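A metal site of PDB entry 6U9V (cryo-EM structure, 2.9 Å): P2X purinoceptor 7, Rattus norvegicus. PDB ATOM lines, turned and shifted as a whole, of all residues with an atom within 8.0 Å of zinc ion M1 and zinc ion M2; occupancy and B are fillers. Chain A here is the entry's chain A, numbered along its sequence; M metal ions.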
ATOM      1  N   GLN A 422     -12.526  -6.654  25.784  1.00  0.00           N
ATOM      2  CA  GLN A 422     -12.378  -7.536  26.934  1.00  0.00           C
ATOM      3  C   GLN A 422     -12.563  -6.779  28.239  1.00  0.00           C
ATOM      4  O   GLN A 422     -13.110  -7.322  29.215  1.00  0.00           O
ATOM      5  CB  GLN A 422     -11.003  -8.221  26.894  1.00  0.00           C
ATOM      6  CG  GLN A 422     -10.970  -9.615  27.502  1.00  0.00           C
ATOM      7  CD  GLN A 422     -11.121  -9.618  29.011  1.00  0.00           C
ATOM      8  OE1 GLN A 422     -10.738  -8.656  29.684  1.00  0.00           O
ATOM      9  NE2 GLN A 422     -11.683 -10.689  29.547  1.00  0.00           N
ATOM     10  N   SER A 473       0.914 -13.848  22.949  1.00  0.00           N
ATOM     11  CA  SER A 473      -0.489 -13.488  22.855  1.00  0.00           C
ATOM     12  C   SER A 473      -0.631 -11.974  22.670  1.00  0.00           C
ATOM     13  O   SER A 473       0.342 -11.225  22.839  1.00  0.00           O
ATOM     14  CB  SER A 473      -1.233 -13.927  24.116  1.00  0.00           C
ATOM     15  OG  SER A 473      -1.118 -15.331  24.302  1.00  0.00           O
ATOM     16  N   PRO A 474      -1.827 -11.487  22.307  1.00  0.00           N
ATOM     17  CA  PRO A 474      -2.037 -10.045  22.188  1.00  0.00           C
ATOM     18  C   PRO A 474      -1.973  -9.279  23.502  1.00  0.00           C
ATOM     19  O   PRO A 474      -2.009  -8.041  23.470  1.00  0.00           O
ATOM     20  CB  PRO A 474      -3.442  -9.950  21.590  1.00  0.00           C
ATOM     21  CG  PRO A 474      -3.681 -11.246  20.934  1.00  0.00           C
ATOM     22  CD  PRO A 474      -2.989 -12.241  21.796  1.00  0.00           C
ATOM     23  N   ASP A 475      -1.905  -9.961  24.644  1.00  0.00           N
ATOM     24  CA  ASP A 475      -1.772  -9.396  25.989  1.00  0.00           C
ATOM     25  C   ASP A 475      -3.094  -8.871  26.552  1.00  0.00           C
ATOM     26  O   ASP A 475      -3.102  -8.395  27.696  1.00  0.00           O
ATOM     27  CB  ASP A 475      -0.733  -8.264  26.057  1.00  0.00           C
ATOM     28  N   TRP A 476      -4.203  -8.945  25.804  1.00  0.00           N
ATOM     29  CA  TRP A 476      -5.524  -8.643  26.353  1.00  0.00           C
ATOM     30  C   TRP A 476      -6.347  -9.887  26.667  1.00  0.00           C
ATOM     31  O   TRP A 476      -7.464  -9.758  27.162  1.00  0.00           O
ATOM     32  CB  TRP A 476      -6.333  -7.726  25.400  1.00  0.00           C
ATOM     33  CG  TRP A 476      -6.349  -8.101  23.944  1.00  0.00           C
ATOM     34  CD1 TRP A 476      -5.687  -7.480  22.929  1.00  0.00           C
ATOM     35  CD2 TRP A 476      -7.086  -9.178  23.330  1.00  0.00           C
ATOM     36  NE1 TRP A 476      -5.959  -8.088  21.731  1.00  0.00           N
ATOM     37  CE2 TRP A 476      -6.816  -9.141  21.954  1.00  0.00           C
ATOM     38  CE3 TRP A 476      -7.951 -10.163  23.818  1.00  0.00           C
ATOM     39  CZ2 TRP A 476      -7.367 -10.052  21.057  1.00  0.00           C
ATOM     40  CZ3 TRP A 476      -8.497 -11.070  22.930  1.00  0.00           C
ATOM     41  CH2 TRP A 476      -8.205 -11.006  21.565  1.00  0.00           C
ATOM     42  N   CYS A 477      -5.820 -11.080  26.385  1.00  0.00           N
ATOM     43  CA  CYS A 477      -6.468 -12.342  26.735  1.00  0.00           C
ATOM     44  C   CYS A 477      -5.727 -12.953  27.915  1.00  0.00           C
ATOM     45  O   CYS A 477      -4.535 -12.689  28.106  1.00  0.00           O
ATOM     46  CB  CYS A 477      -6.472 -13.326  25.557  1.00  0.00           C
ATOM     47  SG  CYS A 477      -5.088 -14.464  25.616  1.00  0.00           S
ATOM     48  N   GLN A 478      -6.434 -13.774  28.690  1.00  0.00           N
ATOM     49  CA  GLN A 478      -5.821 -14.457  29.823  1.00  0.00           C
ATOM     50  C   GLN A 478      -5.416 -15.879  29.450  1.00  0.00           C
ATOM     51  O   GLN A 478      -4.516 -16.463  30.083  1.00  0.00           O
ATOM     52  CB  GLN A 478      -6.773 -14.473  31.014  1.00  0.00           C
ATOM     53  CG  GLN A 478      -7.548 -13.168  31.223  1.00  0.00           C
ATOM     54  CD  GLN A 478      -6.643 -11.953  31.304  1.00  0.00           C
ATOM     55  OE1 GLN A 478      -5.460 -12.058  31.626  1.00  0.00           O
ATOM     56  NE2 GLN A 478      -7.209 -10.789  31.012  1.00  0.00           N
ATOM     57  N   CYS A 479      -6.036 -16.449  28.427  1.00  0.00           N
ATOM     58  CA  CYS A 479      -5.709 -17.784  27.958  1.00  0.00           C
ATOM     59  C   CYS A 479      -4.466 -17.735  27.076  1.00  0.00           C
ATOM     60  O   CYS A 479      -3.741 -16.738  27.091  1.00  0.00           O
ATOM     61  CB  CYS A 479      -6.891 -18.394  27.194  1.00  0.00           C
ATOM     62  SG  CYS A 479      -7.250 -17.611  25.612  1.00  0.00           S
ATOM     63  N   GLY A 480      -4.190 -18.818  26.347  1.00  0.00           N
ATOM     64  CA  GLY A 480      -3.060 -18.885  25.438  1.00  0.00           C
ATOM     65  C   GLY A 480      -3.447 -19.111  23.986  1.00  0.00           C
ATOM     66  O   GLY A 480      -2.615 -18.929  23.090  1.00  0.00           O
ATOM     67  N   ASN A 481      -4.693 -19.500  23.728  1.00  0.00           N
ATOM     68  CA  ASN A 481      -5.131 -19.872  22.385  1.00  0.00           C
ATOM     69  C   ASN A 481      -5.635 -18.698  21.560  1.00  0.00           C
ATOM     70  O   ASN A 481      -6.014 -18.902  20.407  1.00  0.00           O
ATOM     71  CB  ASN A 481      -6.214 -20.943  22.481  1.00  0.00           C
ATOM     72  CG  ASN A 481      -5.696 -22.265  23.003  1.00  0.00           C
ATOM     73  OD1 ASN A 481      -5.400 -23.175  22.228  1.00  0.00           O
ATOM     74  ND2 ASN A 481      -5.573 -22.379  24.318  1.00  0.00           N
ATOM     75  N   CYS A 482      -5.674 -17.483  22.114  1.00  0.00           N
ATOM     76  CA  CYS A 482      -6.122 -16.339  21.339  1.00  0.00           C
ATOM     77  C   CYS A 482      -5.135 -16.029  20.212  1.00  0.00           C
ATOM     78  O   CYS A 482      -4.011 -16.542  20.169  1.00  0.00           O
ATOM     79  CB  CYS A 482      -6.292 -15.109  22.231  1.00  0.00           C
ATOM     80  SG  CYS A 482      -7.856 -15.052  23.149  1.00  0.00           S
ATOM     81  N   LEU A 483      -5.578 -15.193  19.284  1.00  0.00           N
ATOM     82  CA  LEU A 483      -4.791 -14.781  18.132  1.00  0.00           C
ATOM     83  C   LEU A 483      -5.210 -13.368  17.762  1.00  0.00           C
ATOM     84  O   LEU A 483      -6.383 -13.018  17.934  1.00  0.00           O
ATOM     85  CB  LEU A 483      -5.012 -15.733  16.945  1.00  0.00           C
ATOM     86  CG  LEU A 483      -4.111 -15.593  15.715  1.00  0.00           C
ATOM     87  CD1 LEU A 483      -2.733 -16.186  15.988  1.00  0.00           C
ATOM     88  CD2 LEU A 483      -4.749 -16.258  14.509  1.00  0.00           C
ATOM     89  N   LEU A 497     -11.667 -10.012  22.205  1.00  0.00           N
ATOM     90  CA  LEU A 497     -12.365 -10.597  23.336  1.00  0.00           C
ATOM     91  C   LEU A 497     -11.726 -11.936  23.672  1.00  0.00           C
ATOM     92  O   LEU A 497     -11.257 -12.646  22.779  1.00  0.00           O
ATOM     93  CB  LEU A 497     -13.855 -10.772  23.040  1.00  0.00           C
ATOM     94  CG  LEU A 497     -14.734 -11.348  24.156  1.00  0.00           C
ATOM     95  CD1 LEU A 497     -14.771 -10.418  25.360  1.00  0.00           C
ATOM     96  CD2 LEU A 497     -16.139 -11.601  23.633  1.00  0.00           C
ATOM     97  N   CYS A 498     -11.714 -12.257  24.956  1.00  0.00           N
ATOM     98  CA  CYS A 498     -11.134 -13.496  25.464  1.00  0.00           C
ATOM     99  C   CYS A 498     -12.233 -14.369  26.052  1.00  0.00           C
ATOM    100  O   CYS A 498     -13.393 -13.970  26.169  1.00  0.00           O
ATOM    101  CB  CYS A 498     -10.062 -13.204  26.529  1.00  0.00           C
ATOM    102  SG  CYS A 498      -8.956 -14.585  26.865  1.00  0.00           S
ATOM    103  N   CYS A 499     -11.852 -15.589  26.425  1.00  0.00           N
ATOM    104  CA  CYS A 499     -12.792 -16.575  26.930  1.00  0.00           C
ATOM    105  C   CYS A 499     -13.032 -16.467  28.434  1.00  0.00           C
ATOM    106  O   CYS A 499     -13.908 -17.175  28.948  1.00  0.00           O
ATOM    107  CB  CYS A 499     -12.283 -17.987  26.606  1.00  0.00           C
ATOM    108  SG  CYS A 499     -10.626 -18.332  27.200  1.00  0.00           S
ATOM    109  N   ARG A 500     -12.287 -15.619  29.148  1.00  0.00           N
ATOM    110  CA  ARG A 500     -12.451 -15.526  30.590  1.00  0.00           C
ATOM    111  C   ARG A 500     -11.771 -14.261  31.090  1.00  0.00           C
ATOM    112  O   ARG A 500     -10.985 -13.627  30.385  1.00  0.00           O
ATOM    113  CB  ARG A 500     -11.880 -16.764  31.300  1.00  0.00           C
ATOM    114  CG  ARG A 500     -10.447 -17.130  30.930  1.00  0.00           C
ATOM    115  CD  ARG A 500     -10.087 -18.508  31.460  1.00  0.00           C
ATOM    116  NE  ARG A 500     -10.305 -18.607  32.902  1.00  0.00           N
ATOM    117  CZ  ARG A 500     -10.385 -19.752  33.583  1.00  0.00           C
ATOM    118  NH1 ARG A 500     -10.274 -20.932  32.962  1.00  0.00           N
ATOM    119  NH2 ARG A 500     -10.581 -19.723  34.891  1.00  0.00           N
ATOM    120  N   GLY A 504      -6.396 -19.099  33.414  1.00  0.00           N
ATOM    121  CA  GLY A 504      -6.823 -20.437  33.750  1.00  0.00           C
ATOM    122  C   GLY A 504      -6.861 -21.302  32.509  1.00  0.00           C
ATOM    123  O   GLY A 504      -6.157 -21.050  31.523  1.00  0.00           O
ATOM    124  N   GLN A 505      -7.687 -22.334  32.570  1.00  0.00           N
ATOM    125  CA  GLN A 505      -7.858 -23.246  31.447  1.00  0.00           C
ATOM    126  C   GLN A 505      -8.727 -22.607  30.376  1.00  0.00           C
ATOM    127  O   GLN A 505      -9.748 -21.972  30.686  1.00  0.00           O
ATOM    128  CB  GLN A 505      -8.488 -24.561  31.922  1.00  0.00           C
ATOM    129  CG  GLN A 505      -8.624 -25.622  30.834  1.00  0.00           C
ATOM    130  CD  GLN A 505      -9.144 -26.936  31.371  1.00  0.00           C
ATOM    131  OE1 GLN A 505      -9.241 -27.135  32.582  1.00  0.00           O
ATOM    132  NE2 GLN A 505      -9.486 -27.854  30.468  1.00  0.00           N
ATOM    133  N   CYS A 506      -8.325 -22.751  29.120  1.00  0.00           N
ATOM    134  CA  CYS A 506      -9.088 -22.214  28.013  1.00  0.00           C
ATOM    135  C   CYS A 506     -10.326 -23.061  27.752  1.00  0.00           C
ATOM    136  O   CYS A 506     -10.313 -24.283  27.926  1.00  0.00           O
ATOM    137  CB  CYS A 506      -8.228 -22.141  26.749  1.00  0.00           C
ATOM    138  SG  CYS A 506      -8.904 -21.125  25.423  1.00  0.00           S
ATOM    139  N   ILE A 507     -11.409 -22.402  27.341  1.00  0.00           N
ATOM    140  CA  ILE A 507     -12.670 -23.103  27.117  1.00  0.00           C
ATOM    141  C   ILE A 507     -12.566 -24.062  25.941  1.00  0.00           C
ATOM    142  O   ILE A 507     -13.292 -25.061  25.875  1.00  0.00           O
ATOM    143  CB  ILE A 507     -13.814 -22.090  26.919  1.00  0.00           C
ATOM    144  CG1 ILE A 507     -15.177 -22.771  27.062  1.00  0.00           C
ATOM    145  CG2 ILE A 507     -13.716 -21.418  25.555  1.00  0.00           C
ATOM    146  CD1 ILE A 507     -16.348 -21.853  26.832  1.00  0.00           C
ATOM    147  N   THR A 508     -11.674 -23.775  24.985  1.00  0.00           N
ATOM    148  CA  THR A 508     -11.524 -24.658  23.822  1.00  0.00           C
ATOM    149  C   THR A 508     -11.030 -26.052  24.209  1.00  0.00           C
ATOM    150  O   THR A 508     -11.287 -26.998  23.463  1.00  0.00           O
ATOM    151  CB  THR A 508     -10.555 -24.031  22.815  1.00  0.00           C
ATOM    152  OG1 THR A 508     -10.578 -24.782  21.597  1.00  0.00           O
ATOM    153  CG2 THR A 508      -9.125 -24.014  23.363  1.00  0.00           C
ATOM    154  N   THR A 509     -10.340 -26.190  25.338  1.00  0.00           N
ATOM    155  CA  THR A 509      -9.865 -27.491  25.779  1.00  0.00           C
ATOM    156  C   THR A 509     -10.959 -28.353  26.398  1.00  0.00           C
ATOM    157  O   THR A 509     -10.694 -29.504  26.737  1.00  0.00           O
ATOM    158  CB  THR A 509      -8.726 -27.316  26.790  1.00  0.00           C
ATOM    159  OG1 THR A 509      -9.215 -26.613  27.949  1.00  0.00           O
ATOM    160  CG2 THR A 509      -7.574 -26.538  26.175  1.00  0.00           C
ATOM    161  N   TYR A 553     -22.061 -22.328  19.014  1.00  0.00           N
ATOM    162  CA  TYR A 553     -21.389 -21.789  20.195  1.00  0.00           C
ATOM    163  C   TYR A 553     -22.239 -20.712  20.852  1.00  0.00           C
ATOM    164  O   TYR A 553     -22.301 -20.621  22.089  1.00  0.00           O
ATOM    165  CB  TYR A 553     -20.012 -21.246  19.823  1.00  0.00           C
ATOM    166  CG  TYR A 553     -19.194 -20.800  21.026  1.00  0.00           C
ATOM    167  CD1 TYR A 553     -18.402 -21.688  21.718  1.00  0.00           C
ATOM    168  CD2 TYR A 553     -19.237 -19.483  21.462  1.00  0.00           C
ATOM    169  CE1 TYR A 553     -17.663 -21.285  22.814  1.00  0.00           C
ATOM    170  CE2 TYR A 553     -18.511 -19.063  22.547  1.00  0.00           C
ATOM    171  CZ  TYR A 553     -17.718 -19.972  23.221  1.00  0.00           C
ATOM    172  OH  TYR A 553     -16.986 -19.549  24.313  1.00  0.00           O
ATOM    173  N   PRO A 570     -15.068 -15.362  21.449  1.00  0.00           N
ATOM    174  CA  PRO A 570     -13.667 -15.019  21.729  1.00  0.00           C
ATOM    175  C   PRO A 570     -12.753 -15.390  20.580  1.00  0.00           C
ATOM    176  O   PRO A 570     -13.101 -16.169  19.689  1.00  0.00           O
ATOM    177  CB  PRO A 570     -13.355 -15.848  22.972  1.00  0.00           C
ATOM    178  CG  PRO A 570     -14.222 -17.035  22.852  1.00  0.00           C
ATOM    179  CD  PRO A 570     -15.491 -16.548  22.203  1.00  0.00           C
ATOM    180  N   SER A 571     -11.555 -14.803  20.596  1.00  0.00           N
ATOM    181  CA  SER A 571     -10.593 -15.034  19.538  1.00  0.00           C
ATOM    182  C   SER A 571     -10.146 -16.491  19.488  1.00  0.00           C
ATOM    183  O   SER A 571      -9.964 -17.045  18.404  1.00  0.00           O
ATOM    184  CB  SER A 571      -9.391 -14.107  19.714  1.00  0.00           C
ATOM    185  OG  SER A 571      -8.484 -14.232  18.627  1.00  0.00           O
ATOM    186  N   CYS A 572      -9.971 -17.127  20.650  1.00  0.00           N
ATOM    187  CA  CYS A 572      -9.473 -18.495  20.696  1.00  0.00           C
ATOM    188  C   CYS A 572     -10.462 -19.460  20.053  1.00  0.00           C
ATOM    189  O   CYS A 572     -10.069 -20.356  19.292  1.00  0.00           O
ATOM    190  CB  CYS A 572      -9.186 -18.897  22.138  1.00  0.00           C
ATOM    191  SG  CYS A 572     -10.395 -18.311  23.350  1.00  0.00           S
ATOM    192  N   CYS A 573     -11.759 -19.291  20.337  1.00  0.00           N
ATOM    193  CA  CYS A 573     -12.767 -20.162  19.735  1.00  0.00           C
ATOM    194  C   CYS A 573     -13.041 -19.775  18.290  1.00  0.00           C
ATOM    195  O   CYS A 573     -13.248 -20.642  17.436  1.00  0.00           O
ATOM    196  CB  CYS A 573     -14.049 -20.098  20.560  1.00  0.00           C
ATOM    197  SG  CYS A 573     -13.844 -20.591  22.282  1.00  0.00           S
ATOM    198  N   LYS A 576     -10.172 -21.040  16.223  1.00  0.00           N
ATOM    199  CA  LYS A 576     -10.264 -22.492  16.189  1.00  0.00           C
ATOM    200  C   LYS A 576     -11.282 -22.944  15.149  1.00  0.00           C
ATOM    201  O   LYS A 576     -11.012 -23.826  14.329  1.00  0.00           O
ATOM    202  CB  LYS A 576     -10.632 -23.038  17.570  1.00  0.00           C
ATOM    203  CG  LYS A 576      -9.443 -23.280  18.492  1.00  0.00           C
ATOM    204  CD  LYS A 576      -8.757 -24.594  18.168  1.00  0.00           C
ATOM    205  CE  LYS A 576      -7.546 -24.824  19.056  1.00  0.00           C
ATOM    206  NZ  LYS A 576      -7.896 -24.875  20.497  1.00  0.00           N
HETATM  207 ZN    ZN M   1      -9.265 -18.816  25.376  1.00  0.00          ZN
HETATM  208 ZN    ZN M   2      -7.261 -15.284  25.379  1.00  0.00          ZN
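Zinc ion M2 is bound by SG of Cys 482 (2.3 Å), SG of Cys 477 (2.3 Å), SG of Cys 479 (2.3 Å) and SG of Cys 498 (2.4 Å).
Four residues have an atom within 4 Å of zinc ion M1: Cys 479, Cys 499, Cys 506 and Cys 572. Along chain A the residues within 4 Å of zinc ion M1 span positions 479 to 572.
Gln 478 touches zinc ion M2 (N to ZN, 3.7 Å). Five residues have an atom within 4 Å of zinc ion M2: Cys 477, Gln 478, Cys 479, Cys 482 and Cys 498.
SG of Cys 506 lies close to ND2 of Asn 481, at 3.7 Å. O of Cys 506 sits at hydrogen-bond distance from OG1 of Thr 509 (2.6 Å). The side-chain sulfur (SG) of Cys 479 lies close to the backbone NH (N) of Asn 481 (3.7 Å). The side-chain sulfur of Cys 498 sits close to the backbone NH of Gln 478, 3.2 Å away.
Zinc ion M1 is bound by the side-chain sulfur (SG) of Cys 499 (2.3 Å). SG of Cys 506 binds zinc ion M1, at 2.3 Å. Zinc ion M1 is bound by SG of Cys 479, 2.4 Å away. SG of Cys 572 binds zinc ion M1, at 2.4 Å.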
